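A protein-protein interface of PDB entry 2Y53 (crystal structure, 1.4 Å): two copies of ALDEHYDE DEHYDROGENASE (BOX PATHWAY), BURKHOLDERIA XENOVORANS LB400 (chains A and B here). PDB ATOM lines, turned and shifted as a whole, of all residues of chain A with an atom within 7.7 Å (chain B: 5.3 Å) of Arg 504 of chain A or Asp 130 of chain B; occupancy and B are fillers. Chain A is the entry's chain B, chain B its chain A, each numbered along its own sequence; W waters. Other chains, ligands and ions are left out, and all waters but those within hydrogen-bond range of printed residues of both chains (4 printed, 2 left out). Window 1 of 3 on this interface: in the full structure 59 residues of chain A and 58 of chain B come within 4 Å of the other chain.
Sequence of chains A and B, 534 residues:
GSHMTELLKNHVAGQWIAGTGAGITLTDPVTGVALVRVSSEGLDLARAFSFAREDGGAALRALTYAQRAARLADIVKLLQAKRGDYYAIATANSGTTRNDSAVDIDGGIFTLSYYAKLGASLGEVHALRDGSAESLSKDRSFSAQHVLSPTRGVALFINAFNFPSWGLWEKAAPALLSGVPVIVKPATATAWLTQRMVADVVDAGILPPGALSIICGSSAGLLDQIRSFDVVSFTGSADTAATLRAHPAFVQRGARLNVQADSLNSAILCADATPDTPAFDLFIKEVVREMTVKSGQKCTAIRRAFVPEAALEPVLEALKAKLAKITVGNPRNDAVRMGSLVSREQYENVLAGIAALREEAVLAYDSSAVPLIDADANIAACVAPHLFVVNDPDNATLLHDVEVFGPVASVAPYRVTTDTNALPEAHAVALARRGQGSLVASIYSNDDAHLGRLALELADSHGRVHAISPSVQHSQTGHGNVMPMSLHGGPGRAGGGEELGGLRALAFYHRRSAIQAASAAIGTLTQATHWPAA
Water W4 lies within hydrogen-bond range of the side-chain carboxylate (OE2) of Glu 498 of chain A (2.6 Å) and the backbone NH (N) of Arg 512 of chain B (2.8 Å).
Water W2 bridges OH of Tyr 114 of chain A and OE2 of Glu 134 of chain B.
Water W3 lies within hydrogen-bond range of OE2 of Glu 498 of chain A and O of Arg 512 of chain B.
Water W1 lies within hydrogen-bond range of NH2 of Arg 504 of chain A (3.1 Å), O of Ser 132 of chain B (3.4 Å) and OE2 of Glu 134 of chain B (3.4 Å).
No position is printed for both chains.
Of the 8 pairs that touch across the chains among the printed residues, none has its exchanged pair printed and touching as well.
The backbone carbonyl oxygen (O) of Ser 486 of chain A is in hydrogen-bond range of the backbone NH (N) of Gly 501 of chain A.
The side-chain carboxylate of Asp 130 of chain B is in salt-bridge range of the guanidinium group of Arg 512 of chain B.
The backbone carbonyl oxygen (O) of Gly 501 of chain A is in hydrogen-bond range of the guanidinium group (NH1) of Arg 504 of chain A, at 2.9 Å.
The backbone carbonyl oxygen (O) of His 146 of chain B sits at hydrogen-bond distance from the backbone NH (N) of Asp 130 of chain B (3.0 Å).
Arg 504 of chain A touches just these residues of chain B: Asp 130 (3.0 Å) and His 146 (3.4 Å).
Asp 130 of chain B touches one residue of chain A.
Gly 131 of chain B touches none of the printed residues of chain A.
Of the printed residues of chain A, His 146 of chain B touches Met 485, Ser 486, Leu 487 and Arg 504.
Of the printed residues of chain A, Glu 134 of chain B touches Met 485.
Printed residues of chain B within 4 Å of Met 485 of chain A: Glu 134 (3.5 Å) and His 146 (3.5 Å).
Printed residues of chain B within 4 Å of Ser 486 of chain A: His 146 (3.7 Å).
Leu 506 of chain A touches none of the printed residues of chain B.
The nearest printed residue of chain B that does not touch Met 485 of chain A is Ser 132 of chain B (7.5 Å).
ND1 of His 146 of chain B sits at hydrogen-bond distance from NH2 of Arg 504 of chain A (3.4 Å).
The guanidinium group (NE) of Arg 504 of chain A is in salt-bridge range of the side-chain carboxylate (OD2) of Asp 130 of chain B (3.0 Å).
A ring nitrogen (NE2) of His 146 of chain B lies within hydrogen-bond range of the backbone NH of Leu 487 of chain A, at 3.0 Å.
OE1 of Glu 498 of chain A is in salt-bridge range of NH1 of Arg 512 of chain B, 2.5 Å away.
Hydrophobic or aromatic side chains of chain A that line the printed part of chain B: Met 485 and Leu 487.
Printed residues of chain B that touch a printed residue of chain A: Asp 130, Glu 134, His 146 and Arg 512.
Hydrophobic or aromatic side chains of chain B that line the printed part of chain A: His 146.
Met 485 of chain A touches Glu 134 of chain B.
His 146 of chain B touches Met 485 of chain A.
CA of Ser 486 of chain A touches NE2 of His 146 of chain B, 3.7 Å away.
O of Arg 512 of chain B touches CD2 of Leu 487 of chain A, at 3.3 Å.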
ATOM      1  N   TYR A 114       8.676  13.995 -31.953  1.00  0.00           N
ATOM      2  CA  TYR A 114       7.988  13.014 -31.078  1.00  0.00           C
ATOM      3  C   TYR A 114       7.914  13.522 -29.687  1.00  0.00           C
ATOM      4  O   TYR A 114       6.824  13.439 -29.024  1.00  0.00           O
ATOM      5  CB  TYR A 114       8.783  11.650 -31.183  1.00  0.00           C
ATOM      6  CG  TYR A 114       8.430  10.732 -30.102  1.00  0.00           C
ATOM      7  CD1 TYR A 114       7.277   9.968 -30.172  1.00  0.00           C
ATOM      8  CD2 TYR A 114       9.219  10.642 -28.993  1.00  0.00           C
ATOM      9  CE1 TYR A 114       6.897   9.093 -29.152  1.00  0.00           C
ATOM     10  CE2 TYR A 114       8.925   9.779 -28.000  1.00  0.00           C
ATOM     11  CZ  TYR A 114       7.714   9.066 -28.017  1.00  0.00           C
ATOM     12  OH  TYR A 114       7.405   8.172 -27.016  1.00  0.00           O
ATOM     13  N   TYR A 115       8.976  14.126 -29.174  1.00  0.00           N
ATOM     14  CA  TYR A 115       8.951  14.672 -27.793  1.00  0.00           C
ATOM     15  C   TYR A 115       8.088  15.946 -27.724  1.00  0.00           C
ATOM     16  O   TYR A 115       7.442  16.199 -26.673  1.00  0.00           O
ATOM     17  CB  TYR A 115      10.377  14.923 -27.277  1.00  0.00           C
ATOM     18  CG  TYR A 115      10.927  13.630 -26.662  1.00  0.00           C
ATOM     19  CD1 TYR A 115      10.535  13.229 -25.381  1.00  0.00           C
ATOM     20  CD2 TYR A 115      11.790  12.819 -27.390  1.00  0.00           C
ATOM     21  CE1 TYR A 115      10.928  12.022 -24.805  1.00  0.00           C
ATOM     22  CE2 TYR A 115      12.213  11.614 -26.861  1.00  0.00           C
ATOM     23  CZ  TYR A 115      11.796  11.180 -25.586  1.00  0.00           C
ATOM     24  OH  TYR A 115      12.196   9.962 -25.107  1.00  0.00           O
ATOM     25  N   LEU A 118       4.639  14.418 -27.405  1.00  0.00           N
ATOM     26  CA  LEU A 118       4.425  13.790 -26.099  1.00  0.00           C
ATOM     27  C   LEU A 118       4.287  14.880 -25.037  1.00  0.00           C
ATOM     28  O   LEU A 118       3.451  14.791 -24.099  1.00  0.00           O
ATOM     29  CB  LEU A 118       5.662  12.884 -25.835  1.00  0.00           C
ATOM     30  CG  LEU A 118       5.671  11.643 -25.059  1.00  0.00           C
ATOM     31  CD1 LEU A 118       4.651  10.573 -25.578  1.00  0.00           C
ATOM     32  CD2 LEU A 118       7.141  11.205 -25.157  1.00  0.00           C
ATOM     33  N   PRO A 174      14.242  15.558 -24.543  1.00  0.00           N
ATOM     34  CA  PRO A 174      13.708  15.310 -23.218  1.00  0.00           C
ATOM     35  C   PRO A 174      14.306  16.262 -22.160  1.00  0.00           C
ATOM     36  O   PRO A 174      13.562  16.601 -21.216  1.00  0.00           O
ATOM     37  CB  PRO A 174      14.088  13.819 -22.936  1.00  0.00           C
ATOM     38  CG  PRO A 174      15.240  13.532 -23.904  1.00  0.00           C
ATOM     39  CD  PRO A 174      14.892  14.341 -25.120  1.00  0.00           C
ATOM     40  N   PRO A 484      12.357   6.592 -31.031  1.00  0.00           N
ATOM     41  CA  PRO A 484      12.473   7.373 -29.765  1.00  0.00           C
ATOM     42  C   PRO A 484      11.507   6.889 -28.655  1.00  0.00           C
ATOM     43  O   PRO A 484      11.745   7.208 -27.493  1.00  0.00           O
ATOM     44  CB  PRO A 484      12.122   8.818 -30.156  1.00  0.00           C
ATOM     45  CG  PRO A 484      11.271   8.668 -31.414  1.00  0.00           C
ATOM     46  CD  PRO A 484      11.889   7.448 -32.140  1.00  0.00           C
ATOM     47  N   MET A 485      10.476   6.180 -29.056  1.00  0.00           N
ATOM     48  CA  MET A 485       9.554   5.609 -28.067  1.00  0.00           C
ATOM     49  C   MET A 485      10.115   4.390 -27.415  1.00  0.00           C
ATOM     50  O   MET A 485       9.543   3.915 -26.390  1.00  0.00           O
ATOM     51  CB  MET A 485       8.147   5.419 -28.661  1.00  0.00           C
ATOM     52  CG  MET A 485       8.013   4.573 -29.890  1.00  0.00           C
ATOM     53  SD  MET A 485       8.631   5.315 -31.518  1.00  0.00           S
ATOM     54  CE  MET A 485       7.465   6.571 -31.877  1.00  0.00           C
ATOM     55  N   SER A 486      11.217   3.839 -27.889  1.00  0.00           N
ATOM     56  CA  SER A 486      11.833   2.636 -27.348  1.00  0.00           C
ATOM     57  C   SER A 486      13.089   2.987 -26.630  1.00  0.00           C
ATOM     58  O   SER A 486      13.874   3.882 -27.074  1.00  0.00           O
ATOM     59  CB  SER A 486      12.167   1.666 -28.461  1.00  0.00           C
ATOM     60  OG  SER A 486      10.933   1.194 -29.012  1.00  0.00           O
ATOM     61  N   LEU A 487      13.409   2.222 -25.602  1.00  0.00           N
ATOM     62  CA  LEU A 487      14.657   2.383 -24.912  1.00  0.00           C
ATOM     63  C   LEU A 487      15.875   2.262 -25.763  1.00  0.00           C
ATOM     64  O   LEU A 487      15.973   1.360 -26.636  1.00  0.00           O
ATOM     65  CB  LEU A 487      14.724   1.321 -23.800  1.00  0.00           C
ATOM     66  CG  LEU A 487      15.940   1.309 -22.867  1.00  0.00           C
ATOM     67  CD1 LEU A 487      16.011   2.487 -22.065  1.00  0.00           C
ATOM     68  CD2 LEU A 487      16.043   0.016 -21.934  1.00  0.00           C
ATOM     69  N   GLU A 498      20.588   4.386 -20.096  1.00  0.00           N
ATOM     70  CA  GLU A 498      19.251   4.350 -20.654  1.00  0.00           C
ATOM     71  C   GLU A 498      18.933   5.727 -21.173  1.00  0.00           C
ATOM     72  O   GLU A 498      19.182   6.722 -20.418  1.00  0.00           O
ATOM     73  CB  GLU A 498      18.200   3.958 -19.579  1.00  0.00           C
ATOM     74  CG  GLU A 498      18.479   2.563 -19.107  1.00  0.00           C
ATOM     75  CD  GLU A 498      17.358   1.939 -18.304  1.00  0.00           C
ATOM     76  OE1 GLU A 498      16.161   2.271 -18.354  1.00  0.00           O
ATOM     77  OE2 GLU A 498      17.719   0.837 -17.712  1.00  0.00           O
ATOM     78  N   GLU A 499      18.441   5.788 -22.370  1.00  0.00           N
ATOM     79  CA  GLU A 499      17.995   6.986 -23.059  1.00  0.00           C
ATOM     80  C   GLU A 499      16.665   6.669 -23.729  1.00  0.00           C
ATOM     81  O   GLU A 499      16.306   5.492 -23.928  1.00  0.00           O
ATOM     82  CB  GLU A 499      19.010   7.423 -24.100  1.00  0.00           C
ATOM     83  CG  GLU A 499      20.401   7.708 -23.489  1.00  0.00           C
ATOM     84  CD  GLU A 499      21.350   8.142 -24.573  1.00  0.00           C
ATOM     85  OE1 GLU A 499      21.954   7.210 -25.136  1.00  0.00           O
ATOM     86  OE2 GLU A 499      21.442   9.356 -24.827  1.00  0.00           O
ATOM     87  N   LEU A 500      15.983   7.739 -24.101  1.00  0.00           N
ATOM     88  CA  LEU A 500      14.724   7.620 -24.897  1.00  0.00           C
ATOM     89  C   LEU A 500      13.752   6.672 -24.209  1.00  0.00           C
ATOM     90  O   LEU A 500      13.511   6.870 -23.028  1.00  0.00           O
ATOM     91  CB  LEU A 500      15.089   7.194 -26.350  1.00  0.00           C
ATOM     92  CG  LEU A 500      16.048   8.201 -27.069  1.00  0.00           C
ATOM     93  CD1 LEU A 500      16.562   7.634 -28.401  1.00  0.00           C
ATOM     94  CD2 LEU A 500      15.210   9.523 -27.333  1.00  0.00           C
ATOM     95  N   GLY A 501      13.041   5.805 -24.943  1.00  0.00           N
ATOM     96  CA  GLY A 501      11.914   5.120 -24.277  1.00  0.00           C
ATOM     97  C   GLY A 501      10.770   6.046 -23.964  1.00  0.00           C
ATOM     98  O   GLY A 501      10.045   5.780 -22.971  1.00  0.00           O
ATOM     99  N   GLY A 502      10.550   7.024 -24.807  1.00  0.00           N
ATOM    100  CA  GLY A 502       9.411   7.964 -24.624  1.00  0.00           C
ATOM    101  C   GLY A 502       9.540   8.676 -23.314  1.00  0.00           C
ATOM    102  O   GLY A 502      10.525   9.359 -23.021  1.00  0.00           O
ATOM    103  N   LEU A 503       8.471   8.635 -22.512  1.00  0.00           N
ATOM    104  CA  LEU A 503       8.437   9.415 -21.252  1.00  0.00           C
ATOM    105  C   LEU A 503       9.512   8.858 -20.310  1.00  0.00           C
ATOM    106  O   LEU A 503       9.869   9.576 -19.353  1.00  0.00           O
ATOM    107  CB  LEU A 503       7.024   9.295 -20.574  1.00  0.00           C
ATOM    108  CG  LEU A 503       5.945  10.032 -21.318  1.00  0.00           C
ATOM    109  CD1 LEU A 503       4.559   9.646 -20.687  1.00  0.00           C
ATOM    110  CD2 LEU A 503       6.119  11.530 -21.394  1.00  0.00           C
ATOM    111  N   ARG A 504      10.024   7.641 -20.480  1.00  0.00           N
ATOM    112  CA  ARG A 504      11.029   7.131 -19.576  1.00  0.00           C
ATOM    113  C   ARG A 504      12.225   8.042 -19.566  1.00  0.00           C
ATOM    114  O   ARG A 504      12.886   8.191 -18.503  1.00  0.00           O
ATOM    115  CB  ARG A 504      11.501   5.738 -20.041  1.00  0.00           C
ATOM    116  CG  ARG A 504      10.364   4.705 -19.854  1.00  0.00           C
ATOM    117  CD  ARG A 504      10.702   3.349 -20.510  1.00  0.00           C
ATOM    118  NE  ARG A 504       9.552   2.421 -20.507  1.00  0.00           N
ATOM    119  CZ  ARG A 504       8.592   2.479 -21.363  1.00  0.00           C
ATOM    120  NH1 ARG A 504       8.559   3.375 -22.359  1.00  0.00           N
ATOM    121  NH2 ARG A 504       7.620   1.578 -21.197  1.00  0.00           N
ATOM    122  N   ALA A 505      12.494   8.756 -20.653  1.00  0.00           N
ATOM    123  CA  ALA A 505      13.701   9.644 -20.735  1.00  0.00           C
ATOM    124  C   ALA A 505      13.616  10.860 -19.813  1.00  0.00           C
ATOM    125  O   ALA A 505      14.653  11.437 -19.499  1.00  0.00           O
ATOM    126  CB  ALA A 505      13.846  10.133 -22.168  1.00  0.00           C
ATOM    127  N   LEU A 506      12.402  11.204 -19.346  1.00  0.00           N
ATOM    128  CA  LEU A 506      12.304  12.364 -18.475  1.00  0.00           C
ATOM    129  C   LEU A 506      12.920  12.064 -17.144  1.00  0.00           C
ATOM    130  O   LEU A 506      13.348  13.044 -16.424  1.00  0.00           O
ATOM    131  CB  LEU A 506      10.851  12.802 -18.317  1.00  0.00           C
ATOM    132  CG  LEU A 506      10.103  13.028 -19.633  1.00  0.00           C
ATOM    133  CD1 LEU A 506       8.751  13.652 -19.358  1.00  0.00           C
ATOM    134  CD2 LEU A 506      10.855  13.964 -20.556  1.00  0.00           C
ATOM    135  N   ALA A 507      12.969  10.809 -16.638  1.00  0.00           N
ATOM    136  CA  ALA A 507      13.386  10.612 -15.258  1.00  0.00           C
ATOM    137  C   ALA A 507      14.763  11.066 -14.958  1.00  0.00           C
ATOM    138  O   ALA A 507      15.071  11.607 -13.906  1.00  0.00           O
ATOM    139  CB  ALA A 507      13.273   9.096 -14.892  1.00  0.00           C
ATOM    140  N   PHE A 508      15.639  10.941 -15.955  1.00  0.00           N
ATOM    141  CA  PHE A 508      17.038  11.354 -15.808  1.00  0.00           C
ATOM    142  C   PHE A 508      17.194  12.859 -15.532  1.00  0.00           C
ATOM    143  O   PHE A 508      18.186  13.221 -14.882  1.00  0.00           O
ATOM    144  CB  PHE A 508      17.785  10.951 -17.098  1.00  0.00           C
ATOM    145  CG  PHE A 508      19.240  11.277 -17.183  1.00  0.00           C
ATOM    146  CD1 PHE A 508      20.180  10.487 -16.435  1.00  0.00           C
ATOM    147  CD2 PHE A 508      19.684  12.189 -18.061  1.00  0.00           C
ATOM    148  CE1 PHE A 508      21.557  10.801 -16.566  1.00  0.00           C
ATOM    149  CE2 PHE A 508      21.102  12.457 -18.185  1.00  0.00           C
ATOM    150  CZ  PHE A 508      22.045  11.750 -17.431  1.00  0.00           C
ATOM    151  N   TYR A 509      16.199  13.656 -15.964  1.00  0.00           N
ATOM    152  CA  TYR A 509      16.255  15.109 -15.743  1.00  0.00           C
ATOM    153  C   TYR A 509      15.506  15.584 -14.573  1.00  0.00           C
ATOM    154  O   TYR A 509      15.442  16.807 -14.335  1.00  0.00           O
ATOM    155  CB  TYR A 509      15.713  15.786 -17.022  1.00  0.00           C
ATOM    156  CG  TYR A 509      16.598  15.438 -18.227  1.00  0.00           C
ATOM    157  CD1 TYR A 509      17.895  15.983 -18.325  1.00  0.00           C
ATOM    158  CD2 TYR A 509      16.244  14.500 -19.254  1.00  0.00           C
ATOM    159  CE1 TYR A 509      18.759  15.677 -19.395  1.00  0.00           C
ATOM    160  CE2 TYR A 509      17.066  14.182 -20.231  1.00  0.00           C
ATOM    161  CZ  TYR A 509      18.327  14.739 -20.299  1.00  0.00           C
ATOM    162  OH  TYR A 509      19.179  14.413 -21.347  1.00  0.00           O
ATOM    163  N   LEU B 128       8.878  -9.014 -15.822  1.00  0.00           N
ATOM    164  CA  LEU B 128       7.769  -8.070 -15.567  1.00  0.00           C
ATOM    165  C   LEU B 128       7.531  -7.212 -16.748  1.00  0.00           C
ATOM    166  O   LEU B 128       8.435  -6.899 -17.564  1.00  0.00           O
ATOM    167  CB  LEU B 128       8.128  -7.191 -14.378  1.00  0.00           C
ATOM    168  CG  LEU B 128       8.373  -8.021 -13.086  1.00  0.00           C
ATOM    169  CD1 LEU B 128       8.879  -7.005 -11.996  1.00  0.00           C
ATOM    170  CD2 LEU B 128       7.098  -8.757 -12.625  1.00  0.00           C
ATOM    171  N   ARG B 129       6.290  -6.796 -16.970  1.00  0.00           N
ATOM    172  CA  ARG B 129       5.917  -5.887 -18.021  1.00  0.00           C
ATOM    173  C   ARG B 129       6.101  -4.453 -17.614  1.00  0.00           C
ATOM    174  O   ARG B 129       5.587  -4.010 -16.593  1.00  0.00           O
ATOM    175  CB  ARG B 129       4.362  -6.140 -18.295  1.00  0.00           C
ATOM    176  CG  ARG B 129       3.977  -5.299 -19.507  1.00  0.00           C
ATOM    177  CD  ARG B 129       2.465  -5.520 -19.961  1.00  0.00           C
ATOM    178  NE  ARG B 129       1.497  -5.657 -18.838  1.00  0.00           N
ATOM    179  CZ  ARG B 129       1.049  -4.664 -18.124  1.00  0.00           C
ATOM    180  NH1 ARG B 129       1.340  -3.412 -18.390  1.00  0.00           N
ATOM    181  NH2 ARG B 129       0.196  -4.958 -17.157  1.00  0.00           N
ATOM    182  N   ASP B 130       6.849  -3.678 -18.445  1.00  0.00           N
ATOM    183  CA  ASP B 130       7.077  -2.258 -18.170  1.00  0.00           C
ATOM    184  C   ASP B 130       6.218  -1.450 -19.129  1.00  0.00           C
ATOM    185  O   ASP B 130       6.541  -1.250 -20.282  1.00  0.00           O
ATOM    186  CB  ASP B 130       8.572  -1.935 -18.320  1.00  0.00           C
ATOM    187  CG  ASP B 130       8.823  -0.430 -18.311  1.00  0.00           C
ATOM    188  OD1 ASP B 130       8.012   0.445 -18.070  1.00  0.00           O
ATOM    189  OD2 ASP B 130       9.827  -0.058 -18.908  1.00  0.00           O
ATOM    190  N   GLY B 131       5.103  -0.966 -18.646  1.00  0.00           N
ATOM    191  CA  GLY B 131       4.146  -0.234 -19.440  1.00  0.00           C
ATOM    192  C   GLY B 131       3.484  -1.110 -20.486  1.00  0.00           C
ATOM    193  O   GLY B 131       3.328  -2.331 -20.325  1.00  0.00           O
ATOM    194  N   SER B 132       2.938  -0.506 -21.504  1.00  0.00           N
ATOM    195  CA  SER B 132       2.232  -1.327 -22.525  1.00  0.00           C
ATOM    196  C   SER B 132       2.766  -1.164 -23.928  1.00  0.00           C
ATOM    197  O   SER B 132       3.746  -0.321 -24.133  1.00  0.00           O
ATOM    198  CB  SER B 132       0.745  -1.298 -22.496  1.00  0.00           C
ATOM    199  OG  SER B 132       0.554  -0.122 -22.605  1.00  0.00           O
ATOM    200  N   GLU B 134       3.594  -0.217 -27.723  1.00  0.00           N
ATOM    201  CA  GLU B 134       3.398   1.004 -28.519  1.00  0.00           C
ATOM    202  C   GLU B 134       3.537   0.650 -29.965  1.00  0.00           C
ATOM    203  O   GLU B 134       4.498  -0.066 -30.316  1.00  0.00           O
ATOM    204  CB  GLU B 134       4.505   1.949 -28.190  1.00  0.00           C
ATOM    205  CG  GLU B 134       4.335   2.635 -26.925  1.00  0.00           C
ATOM    206  CD  GLU B 134       4.847   4.053 -27.031  1.00  0.00           C
ATOM    207  OE1 GLU B 134       4.772   4.604 -28.110  1.00  0.00           O
ATOM    208  OE2 GLU B 134       5.178   4.613 -25.990  1.00  0.00           O
ATOM    209  N   GLN B 145       7.332  -3.453 -26.875  1.00  0.00           N
ATOM    210  CA  GLN B 145       6.895  -3.689 -25.504  1.00  0.00           C
ATOM    211  C   GLN B 145       8.193  -3.746 -24.655  1.00  0.00           C
ATOM    212  O   GLN B 145       9.079  -4.524 -24.954  1.00  0.00           O
ATOM    213  CB  GLN B 145       6.153  -5.070 -25.418  1.00  0.00           C
ATOM    214  CG  GLN B 145       5.875  -5.479 -23.962  1.00  0.00           C
ATOM    215  CD  GLN B 145       4.892  -4.560 -23.287  1.00  0.00           C
ATOM    216  OE1 GLN B 145       3.722  -4.467 -23.741  1.00  0.00           O
ATOM    217  NE2 GLN B 145       5.236  -3.869 -22.245  1.00  0.00           N
ATOM    218  N   HIS B 146       8.217  -2.949 -23.570  1.00  0.00           N
ATOM    219  CA  HIS B 146       9.353  -3.044 -22.657  1.00  0.00           C
ATOM    220  C   HIS B 146       9.082  -4.066 -21.596  1.00  0.00           C
ATOM    221  O   HIS B 146       7.920  -4.286 -21.136  1.00  0.00           O
ATOM    222  CB  HIS B 146       9.596  -1.670 -21.993  1.00  0.00           C
ATOM    223  CG  HIS B 146      10.028  -0.625 -22.983  1.00  0.00           C
ATOM    224  ND1 HIS B 146       9.158   0.060 -23.799  1.00  0.00           N
ATOM    225  CD2 HIS B 146      11.276  -0.123 -23.261  1.00  0.00           C
ATOM    226  CE1 HIS B 146       9.848   0.934 -24.548  1.00  0.00           C
ATOM    227  NE2 HIS B 146      11.135   0.880 -24.197  1.00  0.00           N
ATOM    228  N   VAL B 147      10.172  -4.706 -21.168  1.00  0.00           N
ATOM    229  CA  VAL B 147      10.131  -5.731 -20.084  1.00  0.00           C
ATOM    230  C   VAL B 147      11.272  -5.481 -19.115  1.00  0.00           C
ATOM    231  O   VAL B 147      12.281  -4.772 -19.463  1.00  0.00           O
ATOM    232  CB  VAL B 147      10.211  -7.163 -20.670  1.00  0.00           C
ATOM    233  CG1 VAL B 147       9.029  -7.456 -21.617  1.00  0.00           C
ATOM    234  CG2 VAL B 147      11.536  -7.412 -21.421  1.00  0.00           C
ATOM    235  N   LEU B 148      11.138  -6.045 -17.936  1.00  0.00           N
ATOM    236  CA  LEU B 148      12.155  -6.043 -16.924  1.00  0.00           C
ATOM    237  C   LEU B 148      12.537  -7.452 -16.618  1.00  0.00           C
ATOM    238  O   LEU B 148      11.638  -8.260 -16.291  1.00  0.00           O
ATOM    239  CB  LEU B 148      11.626  -5.360 -15.656  1.00  0.00           C
ATOM    240  CG  LEU B 148      11.220  -3.882 -15.748  1.00  0.00           C
ATOM    241  CD1 LEU B 148      10.494  -3.462 -14.445  1.00  0.00           C
ATOM    242  CD2 LEU B 148      12.424  -2.979 -15.928  1.00  0.00           C
ATOM    243  N   ARG B 512      16.106  -3.419 -17.972  1.00  0.00           N
ATOM    244  CA  ARG B 512      15.025  -3.039 -18.871  1.00  0.00           C
ATOM    245  C   ARG B 512      15.408  -3.252 -20.340  1.00  0.00           C
ATOM    246  O   ARG B 512      16.512  -3.014 -20.728  1.00  0.00           O
ATOM    247  CB  ARG B 512      14.623  -1.628 -18.590  1.00  0.00           C
ATOM    248  CG  ARG B 512      13.409  -1.144 -19.385  1.00  0.00           C
ATOM    249  CD  ARG B 512      13.255   0.310 -19.197  1.00  0.00           C
ATOM    250  NE  ARG B 512      12.572   0.522 -17.985  1.00  0.00           N
ATOM    251  CZ  ARG B 512      13.138   0.972 -16.880  1.00  0.00           C
ATOM    252  NH1 ARG B 512      14.428   1.238 -16.844  1.00  0.00           N
ATOM    253  NH2 ARG B 512      12.468   1.115 -15.803  1.00  0.00           N
HETATM  254  O   HOH W   1       5.743   2.304 -23.492  1.00  0.00           O
HETATM  255  O   HOH W   2       4.868   7.377 -26.942  1.00  0.00           O
HETATM  256  O   HOH W   3      18.731  -1.251 -19.536  1.00  0.00           O
HETATM  257  O   HOH W   4      17.433  -1.396 -16.506  1.00  0.00           O
